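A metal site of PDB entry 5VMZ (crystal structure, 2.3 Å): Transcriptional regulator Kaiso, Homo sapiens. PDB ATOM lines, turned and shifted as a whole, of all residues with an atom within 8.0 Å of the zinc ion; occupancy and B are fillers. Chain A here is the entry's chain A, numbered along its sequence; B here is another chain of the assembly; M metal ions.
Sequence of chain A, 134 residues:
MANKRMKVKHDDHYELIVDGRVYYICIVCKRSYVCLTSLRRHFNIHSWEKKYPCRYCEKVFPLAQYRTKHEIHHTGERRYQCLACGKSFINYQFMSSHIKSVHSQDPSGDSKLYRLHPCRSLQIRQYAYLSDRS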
ATOM      1  N   ASP A  12     -16.503  18.434 -19.628  1.00  0.00           N
ATOM      2  CA  ASP A  12     -17.417  18.162 -18.523  1.00  0.00           C
ATOM      3  C   ASP A  12     -17.117  16.799 -17.902  1.00  0.00           C
ATOM      4  O   ASP A  12     -17.692  16.412 -16.877  1.00  0.00           O
ATOM      5  CB  ASP A  12     -18.881  18.235 -18.990  1.00  0.00           C
ATOM      6  CG  ASP A  12     -19.236  17.114 -19.948  1.00  0.00           C
ATOM      7  OD1 ASP A  12     -18.347  16.653 -20.694  1.00  0.00           O
ATOM      8  OD2 ASP A  12     -20.423  16.711 -19.948  1.00  0.00           O
ATOM      9  N   ILE A  25     -15.866   9.945 -16.266  1.00  0.00           N
ATOM     10  CA  ILE A  25     -15.906  10.471 -14.915  1.00  0.00           C
ATOM     11  C   ILE A  25     -16.319  11.931 -14.933  1.00  0.00           C
ATOM     12  O   ILE A  25     -15.718  12.763 -15.622  1.00  0.00           O
ATOM     13  CB  ILE A  25     -14.544  10.351 -14.193  1.00  0.00           C
ATOM     14  CG1 ILE A  25     -14.267   8.916 -13.770  1.00  0.00           C
ATOM     15  CG2 ILE A  25     -14.552  11.202 -12.941  1.00  0.00           C
ATOM     16  CD1 ILE A  25     -13.897   7.993 -14.887  1.00  0.00           C
ATOM     17  N   CYS A  26     -17.362  12.223 -14.170  1.00  0.00           N
ATOM     18  CA  CYS A  26     -17.852  13.577 -14.002  1.00  0.00           C
ATOM     19  C   CYS A  26     -16.765  14.473 -13.430  1.00  0.00           C
ATOM     20  O   CYS A  26     -16.152  14.130 -12.422  1.00  0.00           O
ATOM     21  CB  CYS A  26     -19.076  13.556 -13.091  1.00  0.00           C
ATOM     22  SG  CYS A  26     -19.788  15.151 -12.839  1.00  0.00           S
ATOM     23  N   ILE A  27     -16.539  15.621 -14.051  1.00  0.00           N
ATOM     24  CA  ILE A  27     -15.497  16.536 -13.575  1.00  0.00           C
ATOM     25  C   ILE A  27     -15.838  17.084 -12.186  1.00  0.00           C
ATOM     26  O   ILE A  27     -14.944  17.287 -11.355  1.00  0.00           O
ATOM     27  CB  ILE A  27     -15.273  17.707 -14.547  1.00  0.00           C
ATOM     28  CG1 ILE A  27     -14.527  17.213 -15.787  1.00  0.00           C
ATOM     29  CG2 ILE A  27     -14.446  18.800 -13.893  1.00  0.00           C
ATOM     30  CD1 ILE A  27     -13.916  18.328 -16.638  1.00  0.00           C
ATOM     31  N   VAL A  28     -17.124  17.323 -11.942  1.00  0.00           N
ATOM     32  CA  VAL A  28     -17.580  17.930 -10.697  1.00  0.00           C
ATOM     33  C   VAL A  28     -17.535  16.989  -9.488  1.00  0.00           C
ATOM     34  O   VAL A  28     -16.846  17.268  -8.519  1.00  0.00           O
ATOM     35  CB  VAL A  28     -19.014  18.494 -10.828  1.00  0.00           C
ATOM     36  CG1 VAL A  28     -19.597  18.814  -9.451  1.00  0.00           C
ATOM     37  CG2 VAL A  28     -19.024  19.719 -11.718  1.00  0.00           C
ATOM     38  N   CYS A  29     -18.269  15.881  -9.538  1.00  0.00           N
ATOM     39  CA  CYS A  29     -18.389  15.017  -8.354  1.00  0.00           C
ATOM     40  C   CYS A  29     -17.595  13.721  -8.444  1.00  0.00           C
ATOM     41  O   CYS A  29     -17.561  12.952  -7.476  1.00  0.00           O
ATOM     42  CB  CYS A  29     -19.865  14.687  -8.092  1.00  0.00           C
ATOM     43  SG  CYS A  29     -20.641  13.762  -9.426  1.00  0.00           S
ATOM     44  N   LYS A  30     -16.966  13.475  -9.592  1.00  0.00           N
ATOM     45  CA  LYS A  30     -16.136  12.288  -9.838  1.00  0.00           C
ATOM     46  C   LYS A  30     -16.936  10.985  -9.938  1.00  0.00           C
ATOM     47  O   LYS A  30     -16.381   9.900  -9.754  1.00  0.00           O
ATOM     48  CB  LYS A  30     -15.052  12.134  -8.760  1.00  0.00           C
ATOM     49  CG  LYS A  30     -14.307  13.410  -8.389  1.00  0.00           C
ATOM     50  CD  LYS A  30     -13.964  13.420  -6.891  1.00  0.00           C
ATOM     51  CE  LYS A  30     -13.665  14.826  -6.391  1.00  0.00           C
ATOM     52  NZ  LYS A  30     -14.092  15.004  -4.974  1.00  0.00           N
ATOM     53  N   ARG A  31     -18.235  11.077 -10.225  1.00  0.00           N
ATOM     54  CA  ARG A  31     -19.004   9.857 -10.394  1.00  0.00           C
ATOM     55  C   ARG A  31     -18.596   9.187 -11.706  1.00  0.00           C
ATOM     56  O   ARG A  31     -18.227   9.860 -12.667  1.00  0.00           O
ATOM     57  CB  ARG A  31     -20.517  10.125 -10.359  1.00  0.00           C
ATOM     58  CG  ARG A  31     -21.076  10.096  -8.939  1.00  0.00           C
ATOM     59  CD  ARG A  31     -22.539  10.501  -8.903  1.00  0.00           C
ATOM     60  NE  ARG A  31     -22.930  10.904  -7.555  1.00  0.00           N
ATOM     61  CZ  ARG A  31     -23.679  10.162  -6.751  1.00  0.00           C
ATOM     62  NH1 ARG A  31     -24.118   8.976  -7.153  1.00  0.00           N
ATOM     63  NH2 ARG A  31     -23.989  10.609  -5.535  1.00  0.00           N
ATOM     64  N   SER A  32     -18.674   7.861 -11.724  1.00  0.00           N
ATOM     65  CA  SER A  32     -18.191   7.073 -12.849  1.00  0.00           C
ATOM     66  C   SER A  32     -19.348   6.519 -13.676  1.00  0.00           C
ATOM     67  O   SER A  32     -20.325   6.025 -13.117  1.00  0.00           O
ATOM     68  CB  SER A  32     -17.302   5.945 -12.341  1.00  0.00           C
ATOM     69  OG  SER A  32     -17.314   4.831 -13.211  1.00  0.00           O
ATOM     70  N   TYR A  33     -19.238   6.618 -14.995  1.00  0.00           N
ATOM     71  CA  TYR A  33     -20.301   6.150 -15.881  1.00  0.00           C
ATOM     72  C   TYR A  33     -19.726   5.305 -17.015  1.00  0.00           C
ATOM     73  O   TYR A  33     -18.685   5.638 -17.572  1.00  0.00           O
ATOM     74  CB  TYR A  33     -21.077   7.336 -16.453  1.00  0.00           C
ATOM     75  CG  TYR A  33     -21.756   8.103 -15.363  1.00  0.00           C
ATOM     76  CD1 TYR A  33     -21.138   9.207 -14.771  1.00  0.00           C
ATOM     77  CD2 TYR A  33     -23.016   7.710 -14.885  1.00  0.00           C
ATOM     78  CE1 TYR A  33     -21.758   9.908 -13.739  1.00  0.00           C
ATOM     79  CE2 TYR A  33     -23.638   8.384 -13.868  1.00  0.00           C
ATOM     80  CZ  TYR A  33     -23.020   9.485 -13.295  1.00  0.00           C
ATOM     81  OH  TYR A  33     -23.659  10.143 -12.275  1.00  0.00           O
ATOM     82  N   LEU A  39     -23.597  10.076 -18.311  1.00  0.00           N
ATOM     83  CA  LEU A  39     -22.871  11.156 -17.653  1.00  0.00           C
ATOM     84  C   LEU A  39     -23.498  12.480 -18.019  1.00  0.00           C
ATOM     85  O   LEU A  39     -23.592  13.395 -17.199  1.00  0.00           O
ATOM     86  CB  LEU A  39     -21.384  11.174 -18.033  1.00  0.00           C
ATOM     87  CG  LEU A  39     -20.596  12.364 -17.470  1.00  0.00           C
ATOM     88  CD1 LEU A  39     -19.237  11.917 -16.966  1.00  0.00           C
ATOM     89  CD2 LEU A  39     -20.449  13.464 -18.499  1.00  0.00           C
ATOM     90  N   HIS A  42     -26.687  12.841 -16.134  1.00  0.00           N
ATOM     91  CA  HIS A  42     -26.356  13.145 -14.759  1.00  0.00           C
ATOM     92  C   HIS A  42     -25.856  14.579 -14.563  1.00  0.00           C
ATOM     93  O   HIS A  42     -26.226  15.246 -13.587  1.00  0.00           O
ATOM     94  CB  HIS A  42     -25.297  12.174 -14.245  1.00  0.00           C
ATOM     95  CG  HIS A  42     -24.404  12.775 -13.212  1.00  0.00           C
ATOM     96  ND1 HIS A  42     -24.784  12.918 -11.890  1.00  0.00           N
ATOM     97  CD2 HIS A  42     -23.152  13.281 -13.295  1.00  0.00           C
ATOM     98  CE1 HIS A  42     -23.802  13.488 -11.209  1.00  0.00           C
ATOM     99  NE2 HIS A  42     -22.797  13.709 -12.038  1.00  0.00           N
ATOM    100  N   PHE A  43     -24.999  15.034 -15.471  1.00  0.00           N
ATOM    101  CA  PHE A  43     -24.299  16.309 -15.283  1.00  0.00           C
ATOM    102  C   PHE A  43     -25.254  17.505 -15.252  1.00  0.00           C
ATOM    103  O   PHE A  43     -24.890  18.581 -14.785  1.00  0.00           O
ATOM    104  CB  PHE A  43     -23.249  16.488 -16.389  1.00  0.00           C
ATOM    105  CG  PHE A  43     -22.267  17.624 -16.153  1.00  0.00           C
ATOM    106  CD1 PHE A  43     -21.210  17.472 -15.280  1.00  0.00           C
ATOM    107  CD2 PHE A  43     -22.398  18.816 -16.842  1.00  0.00           C
ATOM    108  CE1 PHE A  43     -20.300  18.501 -15.072  1.00  0.00           C
ATOM    109  CE2 PHE A  43     -21.483  19.856 -16.647  1.00  0.00           C
ATOM    110  CZ  PHE A  43     -20.432  19.694 -15.761  1.00  0.00           C
ATOM    111  N   ASN A  44     -26.487  17.324 -15.718  1.00  0.00           N
ATOM    112  CA  ASN A  44     -27.432  18.450 -15.724  1.00  0.00           C
ATOM    113  C   ASN A  44     -27.750  18.873 -14.298  1.00  0.00           C
ATOM    114  O   ASN A  44     -28.103  20.022 -14.047  1.00  0.00           O
ATOM    115  CB  ASN A  44     -28.710  18.119 -16.474  1.00  0.00           C
ATOM    116  CG  ASN A  44     -29.535  19.357 -16.770  1.00  0.00           C
ATOM    117  OD1 ASN A  44     -29.068  20.273 -17.455  1.00  0.00           O
ATOM    118  ND2 ASN A  44     -30.746  19.399 -16.250  1.00  0.00           N
ATOM    119  N   ILE A  45     -27.599  17.929 -13.385  1.00  0.00           N
ATOM    120  CA  ILE A  45     -27.755  18.182 -11.956  1.00  0.00           C
ATOM    121  C   ILE A  45     -26.818  19.292 -11.459  1.00  0.00           C
ATOM    122  O   ILE A  45     -27.209  20.089 -10.602  1.00  0.00           O
ATOM    123  CB  ILE A  45     -27.499  16.891 -11.176  1.00  0.00           C
ATOM    124  CG1 ILE A  45     -28.728  15.987 -11.285  1.00  0.00           C
ATOM    125  CG2 ILE A  45     -27.145  17.175  -9.725  1.00  0.00           C
ATOM    126  CD1 ILE A  45     -28.498  14.586 -10.778  1.00  0.00           C
ATOM    127  N   HIS A  46     -25.614  19.359 -12.012  1.00  0.00           N
ATOM    128  CA  HIS A  46     -24.650  20.418 -11.647  1.00  0.00           C
ATOM    129  C   HIS A  46     -24.909  21.725 -12.400  1.00  0.00           C
ATOM    130  O   HIS A  46     -24.867  22.810 -11.821  1.00  0.00           O
ATOM    131  CB  HIS A  46     -23.217  19.955 -11.916  1.00  0.00           C
ATOM    132  CG  HIS A  46     -22.851  18.654 -11.257  1.00  0.00           C
ATOM    133  ND1 HIS A  46     -23.071  18.414  -9.918  1.00  0.00           N
ATOM    134  CD2 HIS A  46     -22.301  17.522 -11.758  1.00  0.00           C
ATOM    135  CE1 HIS A  46     -22.651  17.186  -9.622  1.00  0.00           C
ATOM    136  NE2 HIS A  46     -22.181  16.635 -10.725  1.00  0.00           N
ATOM    137  N1  5CM B   8     -28.976   4.751 -13.941  1.00  0.00           N
ATOM    138  C2  5CM B   8     -30.010   3.713 -13.880  1.00  0.00           C
ATOM    139  N3  5CM B   8     -31.416   4.107 -13.832  1.00  0.00           N
ATOM    140  C4  5CM B   8     -31.781   5.460 -13.828  1.00  0.00           C
ATOM    141  C5  5CM B   8     -30.743   6.489 -13.887  1.00  0.00           C
ATOM    142  C5A 5CM B   8     -31.156   7.953 -13.885  1.00  0.00           C
ATOM    143  C6  5CM B   8     -29.334   6.116 -13.940  1.00  0.00           C
ATOM    144  O2  5CM B   8     -29.691   2.527 -13.889  1.00  0.00           O
ATOM    145  N4  5CM B   8     -33.158   5.833 -13.775  1.00  0.00           N
ATOM    146  C1' 5CM B   8     -27.592   4.329 -13.983  1.00  0.00           C
ATOM    147  C2' 5CM B   8     -26.612   5.414 -14.555  1.00  0.00           C
ATOM    148  C3' 5CM B   8     -25.315   4.790 -14.125  1.00  0.00           C
ATOM    149  C4' 5CM B   8     -25.554   4.294 -12.895  1.00  0.00           C
ATOM    150  O4' 5CM B   8     -27.155   4.178 -12.790  1.00  0.00           O
ATOM    151  O3' 5CM B   8     -25.138   3.612 -15.002  1.00  0.00           O
ATOM    152  C5' 5CM B   8     -25.032   5.168 -11.794  1.00  0.00           C
ATOM    153  O5' 5CM B   8     -25.518   6.485 -12.017  1.00  0.00           O
ATOM    154  P   5CM B   8     -25.417   7.533 -10.827  1.00  0.00           P
ATOM    155  OP1 5CM B   8     -24.068   7.380 -10.139  1.00  0.00           O
ATOM    156  OP2 5CM B   8     -25.716   8.921 -11.332  1.00  0.00           O
HETATM  157 ZN    ZN M   1     -21.334  14.866 -11.207  1.00  0.00          ZN
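SG of Cys 29 lies close to N of Arg 31, at 3.7 Å.
SG of Cys 26 lies close to N of Val 28 (3.6 Å).
ND1 of His 42 sits close to OH of Tyr 33 (3.0 Å).
The backbone NH of Cys 26 lies within hydrogen-bond range of the backbone carbonyl oxygen of Arg 31 (2.9 Å).
NE2 of His 46 binds the zinc ion, 2.0 Å away.
NE2 of His 42 binds the zinc ion, 2.0 Å away.
SG of Cys 29 is bound to the zinc ion (2.2 Å).
SG of Cys 26 binds the zinc ion (2.3 Å).
The zinc ion has four donor atoms within binding distance.
The nearest printed residue that does not touch the zinc ion is Val 28 (4.3 Å).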
